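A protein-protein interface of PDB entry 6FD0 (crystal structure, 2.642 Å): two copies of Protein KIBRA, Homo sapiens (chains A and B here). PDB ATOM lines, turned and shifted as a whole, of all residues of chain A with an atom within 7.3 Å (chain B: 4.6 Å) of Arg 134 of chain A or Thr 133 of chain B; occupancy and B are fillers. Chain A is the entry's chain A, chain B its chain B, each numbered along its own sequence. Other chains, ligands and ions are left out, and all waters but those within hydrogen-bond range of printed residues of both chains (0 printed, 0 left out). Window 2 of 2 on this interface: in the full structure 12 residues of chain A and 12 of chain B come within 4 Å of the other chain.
Among the printed residues, merely in contact across the chains: Glu 124 of chain A with Ser 132 of chain B.
Arg 134 of chain A touches Thr 133 of chain B, but with the chains exchanged Thr 133 of chain A does not touch Arg 134 of chain B (4.4 Å).
Arg 134 of chain B touches its own counterpart, Arg 134 of chain A.
7 positions are printed for both chains.
Arg 134 of chain A touches just these residues of chain B: Thr 133 (3.4 Å) and Arg 134 (3.2 Å).
Printed residues of chain A within 4 Å of Thr 133 of chain B: Glu 124 (2.7 Å) and Arg 134 (3.4 Å).
Printed residues of chain A within 4 Å of Arg 134 of chain B: Glu 124 (3.5 Å) and Arg 134 (3.2 Å).
Of the printed residues of chain A, Ser 132 of chain B touches Glu 124 (3.3 Å).
Of the printed residues of chain B, Glu 124 of chain A touches Arg 131, Ser 132, Thr 133 and Arg 134.
Ile 35 of chain A touches none of the printed residues of chain B.
Ile 19 of chain A touches none of the printed residues of chain B.
The nearest printed residue of chain A that does not touch Thr 133 of chain B is Tyr 136 of chain A (7.7 Å).
The nearest printed residue of chain A that does not touch Arg 131 of chain B is Arg 134 of chain A (7.6 Å).
N of Ile 19 of chain A is in hydrogen-bond range of O of Arg 134 of chain A, 3.0 Å away.
The side-chain carboxylate (OE1) of Glu 124 of chain A lies within salt-bridge range of the guanidinium group (NH1) of Arg 134 of chain A, 3.8 Å away.
The backbone NH (N) of Ile 19 of chain B is in hydrogen-bond range of the backbone carbonyl oxygen (O) of Arg 134 of chain B (2.8 Å).
Of the 8 printed residues of chain B, 4 touch a printed residue of chain A.
Of the 16 printed residues of chain A, 2 touch a printed residue of chain B.
Among the printed residues, Asp or Glu carboxylates within 4 Å of a Lys or Arg side-chain nitrogen of the other chain: Glu 124 of chain A with Arg 134 of chain B.
The side-chain carboxylate of Glu 124 of chain A is in hydrogen-bond range of the backbone NH of Thr 133 of chain B.
The guanidinium group (NH2) of Arg 134 of chain B is in salt-bridge range of the side-chain carboxylate (OE1) of Glu 124 of chain A (3.5 Å).
NH1 of Arg 134 of chain A lies within hydrogen-bond range of O of Thr 133 of chain B (3.4 Å).
The backbone carbonyl oxygen (O) of Arg 131 of chain B lies close to the side-chain carboxylate (OE2) of Glu 124 of chain A, 3.2 Å away.
NE of Arg 134 of chain B lies close to NE of Arg 134 of chain A, at 3.4 Å.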
ATOM      1  N   ILE A  17     -10.886 -27.833  22.129  1.00  0.00           N
ATOM      2  CA  ILE A  17     -10.435 -27.128  20.933  1.00  0.00           C
ATOM      3  C   ILE A  17     -11.648 -26.608  20.171  1.00  0.00           C
ATOM      4  O   ILE A  17     -12.644 -27.322  20.007  1.00  0.00           O
ATOM      5  CB  ILE A  17      -9.571 -28.032  20.029  1.00  0.00           C
ATOM      6  CG1 ILE A  17      -8.992 -27.223  18.869  1.00  0.00           C
ATOM      7  CG2 ILE A  17     -10.375 -29.210  19.499  1.00  0.00           C
ATOM      8  CD1 ILE A  17      -7.773 -27.848  18.272  1.00  0.00           C
ATOM      9  N   GLN A  18     -11.557 -25.364  19.700  1.00  0.00           N
ATOM     10  CA  GLN A  18     -12.654 -24.688  19.020  1.00  0.00           C
ATOM     11  C   GLN A  18     -12.418 -24.713  17.517  1.00  0.00           C
ATOM     12  O   GLN A  18     -11.372 -24.258  17.038  1.00  0.00           O
ATOM     13  CB  GLN A  18     -12.782 -23.244  19.501  1.00  0.00           C
ATOM     14  CG  GLN A  18     -13.995 -22.513  18.940  1.00  0.00           C
ATOM     15  CD  GLN A  18     -14.107 -21.098  19.455  1.00  0.00           C
ATOM     16  OE1 GLN A  18     -13.208 -20.282  19.263  1.00  0.00           O
ATOM     17  NE2 GLN A  18     -15.208 -20.802  20.126  1.00  0.00           N
ATOM     18  N   ILE A  19     -13.402 -25.217  16.777  1.00  0.00           N
ATOM     19  CA  ILE A  19     -13.267 -25.404  15.340  1.00  0.00           C
ATOM     20  C   ILE A  19     -14.547 -24.945  14.656  1.00  0.00           C
ATOM     21  O   ILE A  19     -15.652 -25.151  15.171  1.00  0.00           O
ATOM     22  CB  ILE A  19     -12.953 -26.874  14.995  1.00  0.00           C
ATOM     23  CG1 ILE A  19     -11.710 -27.338  15.758  1.00  0.00           C
ATOM     24  CG2 ILE A  19     -12.730 -27.022  13.500  1.00  0.00           C
ATOM     25  CD1 ILE A  19     -11.348 -28.796  15.546  1.00  0.00           C
ATOM     26  N   ALA A  20     -14.388 -24.316  13.495  1.00  0.00           N
ATOM     27  CA  ALA A  20     -15.497 -23.923  12.639  1.00  0.00           C
ATOM     28  C   ALA A  20     -15.497 -24.794  11.391  1.00  0.00           C
ATOM     29  O   ALA A  20     -14.434 -25.171  10.889  1.00  0.00           O
ATOM     30  CB  ALA A  20     -15.405 -22.448  12.244  1.00  0.00           C
ATOM     31  N   LEU A  21     -16.696 -25.118  10.899  1.00  0.00           N
ATOM     32  CA  LEU A  21     -16.866 -25.994   9.745  1.00  0.00           C
ATOM     33  C   LEU A  21     -17.911 -25.408   8.806  1.00  0.00           C
ATOM     34  O   LEU A  21     -19.030 -25.098   9.228  1.00  0.00           O
ATOM     35  CB  LEU A  21     -17.280 -27.407  10.177  1.00  0.00           C
ATOM     36  CG  LEU A  21     -16.360 -28.122  11.170  1.00  0.00           C
ATOM     37  CD1 LEU A  21     -16.978 -29.439  11.544  1.00  0.00           C
ATOM     38  CD2 LEU A  21     -14.957 -28.333  10.611  1.00  0.00           C
ATOM     39  N   LEU A  33     -11.477 -24.556  10.011  1.00  0.00           N
ATOM     40  CA  LEU A  33     -10.788 -23.482  10.722  1.00  0.00           C
ATOM     41  C   LEU A  33     -10.486 -23.939  12.146  1.00  0.00           C
ATOM     42  O   LEU A  33     -11.401 -24.122  12.956  1.00  0.00           O
ATOM     43  CB  LEU A  33     -11.626 -22.207  10.733  1.00  0.00           C
ATOM     44  CG  LEU A  33     -11.060 -21.061  11.573  1.00  0.00           C
ATOM     45  CD1 LEU A  33      -9.791 -20.474  10.956  1.00  0.00           C
ATOM     46  CD2 LEU A  33     -12.114 -20.004  11.747  1.00  0.00           C
ATOM     47  N   ILE A  35      -9.448 -22.686  15.448  1.00  0.00           N
ATOM     48  CA  ILE A  35      -9.468 -21.350  16.036  1.00  0.00           C
ATOM     49  C   ILE A  35      -8.564 -21.284  17.257  1.00  0.00           C
ATOM     50  O   ILE A  35      -7.608 -20.503  17.286  1.00  0.00           O
ATOM     51  CB  ILE A  35     -10.897 -20.920  16.404  1.00  0.00           C
ATOM     52  CG1 ILE A  35     -11.777 -20.910  15.150  1.00  0.00           C
ATOM     53  CG2 ILE A  35     -10.874 -19.534  17.066  1.00  0.00           C
ATOM     54  CD1 ILE A  35     -13.210 -20.555  15.405  1.00  0.00           C
ATOM     55  N   GLN A  36      -8.859 -22.077  18.281  1.00  0.00           N
ATOM     56  CA  GLN A  36      -8.104 -21.929  19.511  1.00  0.00           C
ATOM     57  C   GLN A  36      -8.184 -23.199  20.338  1.00  0.00           C
ATOM     58  O   GLN A  36      -9.163 -23.945  20.275  1.00  0.00           O
ATOM     59  CB  GLN A  36      -8.610 -20.734  20.326  1.00  0.00           C
ATOM     60  CG  GLN A  36     -10.072 -20.819  20.719  1.00  0.00           C
ATOM     61  CD  GLN A  36     -10.538 -19.610  21.512  1.00  0.00           C
ATOM     62  OE1 GLN A  36      -9.774 -19.016  22.274  1.00  0.00           O
ATOM     63  NE2 GLN A  36     -11.799 -19.241  21.334  1.00  0.00           N
ATOM     64  N   ILE A 120     -14.677 -36.674  15.057  1.00  0.00           N
ATOM     65  CA  ILE A 120     -15.853 -35.811  14.989  1.00  0.00           C
ATOM     66  C   ILE A 120     -16.668 -36.190  13.761  1.00  0.00           C
ATOM     67  O   ILE A 120     -16.160 -36.135  12.633  1.00  0.00           O
ATOM     68  CB  ILE A 120     -15.466 -34.323  14.932  1.00  0.00           C
ATOM     69  CG1 ILE A 120     -14.483 -33.979  16.061  1.00  0.00           C
ATOM     70  CG2 ILE A 120     -16.724 -33.442  14.993  1.00  0.00           C
ATOM     71  CD1 ILE A 120     -13.906 -32.572  15.979  1.00  0.00           C
ATOM     72  N   SER A 121     -17.930 -36.553  13.976  1.00  0.00           N
ATOM     73  CA  SER A 121     -18.846 -36.797  12.868  1.00  0.00           C
ATOM     74  C   SER A 121     -19.122 -35.523  12.087  1.00  0.00           C
ATOM     75  O   SER A 121     -19.404 -34.469  12.663  1.00  0.00           O
ATOM     76  CB  SER A 121     -20.177 -37.339  13.365  1.00  0.00           C
ATOM     77  OG  SER A 121     -21.145 -37.192  12.340  1.00  0.00           O
ATOM     78  N   GLU A 124     -23.376 -33.663  10.480  1.00  0.00           N
ATOM     79  CA  GLU A 124     -24.086 -32.432  10.782  1.00  0.00           C
ATOM     80  C   GLU A 124     -23.634 -31.257   9.927  1.00  0.00           C
ATOM     81  O   GLU A 124     -24.326 -30.230   9.893  1.00  0.00           O
ATOM     82  CB  GLU A 124     -23.912 -32.081  12.263  1.00  0.00           C
ATOM     83  CG  GLU A 124     -24.493 -33.123  13.207  1.00  0.00           C
ATOM     84  CD  GLU A 124     -24.910 -32.526  14.524  1.00  0.00           C
ATOM     85  OE1 GLU A 124     -24.274 -31.544  14.955  1.00  0.00           O
ATOM     86  OE2 GLU A 124     -25.885 -33.033  15.117  1.00  0.00           O
ATOM     87  N   SER A 132     -20.717 -23.994  11.340  1.00  0.00           N
ATOM     88  CA  SER A 132     -20.840 -24.553  12.680  1.00  0.00           C
ATOM     89  C   SER A 132     -19.566 -24.244  13.454  1.00  0.00           C
ATOM     90  O   SER A 132     -18.464 -24.463  12.948  1.00  0.00           O
ATOM     91  CB  SER A 132     -21.079 -26.062  12.632  1.00  0.00           C
ATOM     92  OG  SER A 132     -19.990 -26.739  12.027  1.00  0.00           O
ATOM     93  N   THR A 133     -19.716 -23.714  14.665  1.00  0.00           N
ATOM     94  CA  THR A 133     -18.582 -23.348  15.507  1.00  0.00           C
ATOM     95  C   THR A 133     -18.793 -23.985  16.872  1.00  0.00           C
ATOM     96  O   THR A 133     -19.681 -23.566  17.621  1.00  0.00           O
ATOM     97  CB  THR A 133     -18.454 -21.832  15.627  1.00  0.00           C
ATOM     98  OG1 THR A 133     -18.573 -21.239  14.325  1.00  0.00           O
ATOM     99  CG2 THR A 133     -17.107 -21.460  16.249  1.00  0.00           C
ATOM    100  N   ARG A 134     -17.978 -24.986  17.195  1.00  0.00           N
ATOM    101  CA  ARG A 134     -18.153 -25.751  18.420  1.00  0.00           C
ATOM    102  C   ARG A 134     -16.816 -25.951  19.112  1.00  0.00           C
ATOM    103  O   ARG A 134     -15.746 -25.832  18.507  1.00  0.00           O
ATOM    104  CB  ARG A 134     -18.764 -27.133  18.164  1.00  0.00           C
ATOM    105  CG  ARG A 134     -20.149 -27.162  17.560  1.00  0.00           C
ATOM    106  CD  ARG A 134     -20.561 -28.619  17.374  1.00  0.00           C
ATOM    107  NE  ARG A 134     -20.822 -29.294  18.646  1.00  0.00           N
ATOM    108  CZ  ARG A 134     -21.319 -30.525  18.762  1.00  0.00           C
ATOM    109  NH1 ARG A 134     -21.628 -31.236  17.678  1.00  0.00           N
ATOM    110  NH2 ARG A 134     -21.513 -31.044  19.966  1.00  0.00           N
ATOM    111  N   TRP A 135     -16.903 -26.275  20.396  1.00  0.00           N
ATOM    112  CA  TRP A 135     -15.770 -26.729  21.185  1.00  0.00           C
ATOM    113  C   TRP A 135     -15.796 -28.249  21.287  1.00  0.00           C
ATOM    114  O   TRP A 135     -16.854 -28.845  21.512  1.00  0.00           O
ATOM    115  CB  TRP A 135     -15.822 -26.142  22.587  1.00  0.00           C
ATOM    116  CG  TRP A 135     -15.411 -24.731  22.721  1.00  0.00           C
ATOM    117  CD1 TRP A 135     -16.226 -23.649  22.758  1.00  0.00           C
ATOM    118  CD2 TRP A 135     -14.076 -24.241  22.899  1.00  0.00           C
ATOM    119  NE1 TRP A 135     -15.485 -22.503  22.935  1.00  0.00           N
ATOM    120  CE2 TRP A 135     -14.160 -22.841  23.022  1.00  0.00           C
ATOM    121  CE3 TRP A 135     -12.815 -24.848  22.957  1.00  0.00           C
ATOM    122  CZ2 TRP A 135     -13.035 -22.038  23.196  1.00  0.00           C
ATOM    123  CZ3 TRP A 135     -11.701 -24.047  23.131  1.00  0.00           C
ATOM    124  CH2 TRP A 135     -11.820 -22.660  23.253  1.00  0.00           C
ATOM    125  N   TYR A 136     -14.627 -28.872  21.143  1.00  0.00           N
ATOM    126  CA  TYR A 136     -14.506 -30.326  21.179  1.00  0.00           C
ATOM    127  C   TYR A 136     -13.437 -30.716  22.188  1.00  0.00           C
ATOM    128  O   TYR A 136     -12.349 -30.136  22.208  1.00  0.00           O
ATOM    129  CB  TYR A 136     -14.166 -30.904  19.795  1.00  0.00           C
ATOM    130  CG  TYR A 136     -15.160 -30.544  18.700  1.00  0.00           C
ATOM    131  CD1 TYR A 136     -16.320 -31.286  18.518  1.00  0.00           C
ATOM    132  CD2 TYR A 136     -14.937 -29.467  17.850  1.00  0.00           C
ATOM    133  CE1 TYR A 136     -17.227 -30.968  17.533  1.00  0.00           C
ATOM    134  CE2 TYR A 136     -15.840 -29.139  16.863  1.00  0.00           C
ATOM    135  CZ  TYR A 136     -16.983 -29.895  16.707  1.00  0.00           C
ATOM    136  OH  TYR A 136     -17.885 -29.571  15.719  1.00  0.00           O
ATOM    137  N   GLN B  18     -29.308 -30.739  26.440  1.00  0.00           N
ATOM    138  CA  GLN B  18     -28.943 -31.196  25.104  1.00  0.00           C
ATOM    139  C   GLN B  18     -30.127 -31.019  24.161  1.00  0.00           C
ATOM    140  O   GLN B  18     -31.246 -31.442  24.474  1.00  0.00           O
ATOM    141  CB  GLN B  18     -28.509 -32.663  25.128  1.00  0.00           C
ATOM    142  CG  GLN B  18     -28.184 -33.231  23.757  1.00  0.00           C
ATOM    143  CD  GLN B  18     -27.611 -34.621  23.822  1.00  0.00           C
ATOM    144  OE1 GLN B  18     -28.224 -35.529  24.374  1.00  0.00           O
ATOM    145  NE2 GLN B  18     -26.424 -34.796  23.256  1.00  0.00           N
ATOM    146  N   ILE B  19     -29.874 -30.403  23.007  1.00  0.00           N
ATOM    147  CA  ILE B  19     -30.927 -30.071  22.060  1.00  0.00           C
ATOM    148  C   ILE B  19     -30.463 -30.421  20.657  1.00  0.00           C
ATOM    149  O   ILE B  19     -29.281 -30.290  20.319  1.00  0.00           O
ATOM    150  CB  ILE B  19     -31.327 -28.577  22.143  1.00  0.00           C
ATOM    151  CG1 ILE B  19     -31.773 -28.220  23.563  1.00  0.00           C
ATOM    152  CG2 ILE B  19     -32.436 -28.252  21.122  1.00  0.00           C
ATOM    153  CD1 ILE B  19     -31.921 -26.742  23.798  1.00  0.00           C
ATOM    154  N   ALA B  20     -31.407 -30.865  19.833  1.00  0.00           N
ATOM    155  CA  ALA B  20     -31.179 -31.112  18.420  1.00  0.00           C
ATOM    156  C   ALA B  20     -32.144 -30.258  17.611  1.00  0.00           C
ATOM    157  O   ALA B  20     -33.309 -30.094  17.988  1.00  0.00           O
ATOM    158  CB  ALA B  20     -31.360 -32.591  18.072  1.00  0.00           C
ATOM    159  N   ILE B  35     -33.899 -33.099  24.521  1.00  0.00           N
ATOM    160  CA  ILE B  35     -33.378 -34.448  24.678  1.00  0.00           C
ATOM    161  C   ILE B  35     -33.141 -34.799  26.143  1.00  0.00           C
ATOM    162  O   ILE B  35     -33.601 -35.833  26.621  1.00  0.00           O
ATOM    163  CB  ILE B  35     -32.093 -34.626  23.839  1.00  0.00           C
ATOM    164  CG1 ILE B  35     -32.402 -34.410  22.361  1.00  0.00           C
ATOM    165  CG2 ILE B  35     -31.542 -36.018  24.042  1.00  0.00           C
ATOM    166  CD1 ILE B  35     -31.188 -34.390  21.461  1.00  0.00           C
ATOM    167  N   ARG B 131     -29.324 -32.280  10.835  1.00  0.00           N
ATOM    168  CA  ARG B 131     -29.598 -32.095  12.250  1.00  0.00           C
ATOM    169  C   ARG B 131     -28.369 -31.522  12.951  1.00  0.00           C
ATOM    170  O   ARG B 131     -27.231 -31.751  12.538  1.00  0.00           O
ATOM    171  CB  ARG B 131     -30.007 -33.435  12.871  1.00  0.00           C
ATOM    172  CG  ARG B 131     -30.655 -33.348  14.246  1.00  0.00           C
ATOM    173  CD  ARG B 131     -31.094 -34.723  14.768  1.00  0.00           C
ATOM    174  NE  ARG B 131     -32.256 -35.253  14.054  1.00  0.00           N
ATOM    175  CZ  ARG B 131     -32.200 -36.046  12.985  1.00  0.00           C
ATOM    176  NH1 ARG B 131     -31.032 -36.417  12.479  1.00  0.00           N
ATOM    177  NH2 ARG B 131     -33.322 -36.470  12.419  1.00  0.00           N
ATOM    178  N   SER B 132     -28.605 -30.745  14.007  1.00  0.00           N
ATOM    179  CA  SER B 132     -27.523 -30.134  14.774  1.00  0.00           C
ATOM    180  C   SER B 132     -27.782 -30.379  16.253  1.00  0.00           C
ATOM    181  O   SER B 132     -28.690 -29.773  16.834  1.00  0.00           O
ATOM    182  CB  SER B 132     -27.403 -28.636  14.490  1.00  0.00           C
ATOM    183  OG  SER B 132     -28.177 -27.880  15.405  1.00  0.00           O
ATOM    184  N   THR B 133     -26.974 -31.253  16.855  1.00  0.00           N
ATOM    185  CA  THR B 133     -27.118 -31.653  18.249  1.00  0.00           C
ATOM    186  C   THR B 133     -26.019 -30.983  19.066  1.00  0.00           C
ATOM    187  O   THR B 133     -24.856 -30.967  18.654  1.00  0.00           O
ATOM    188  CB  THR B 133     -27.046 -33.178  18.385  1.00  0.00           C
ATOM    189  OG1 THR B 133     -27.724 -33.800  17.280  1.00  0.00           O
ATOM    190  CG2 THR B 133     -27.697 -33.632  19.681  1.00  0.00           C
ATOM    191  N   ARG B 134     -26.387 -30.432  20.221  1.00  0.00           N
ATOM    192  CA  ARG B 134     -25.478 -29.597  20.993  1.00  0.00           C
ATOM    193  C   ARG B 134     -25.968 -29.536  22.432  1.00  0.00           C
ATOM    194  O   ARG B 134     -27.150 -29.751  22.713  1.00  0.00           O
ATOM    195  CB  ARG B 134     -25.389 -28.186  20.391  1.00  0.00           C
ATOM    196  CG  ARG B 134     -24.005 -27.552  20.399  1.00  0.00           C
ATOM    197  CD  ARG B 134     -23.746 -26.789  19.111  1.00  0.00           C
ATOM    198  NE  ARG B 134     -23.779 -27.686  17.956  1.00  0.00           N
ATOM    199  CZ  ARG B 134     -23.444 -27.339  16.715  1.00  0.00           C
ATOM    200  NH1 ARG B 134     -23.023 -26.109  16.448  1.00  0.00           N
ATOM    201  NH2 ARG B 134     -23.516 -28.237  15.738  1.00  0.00           N
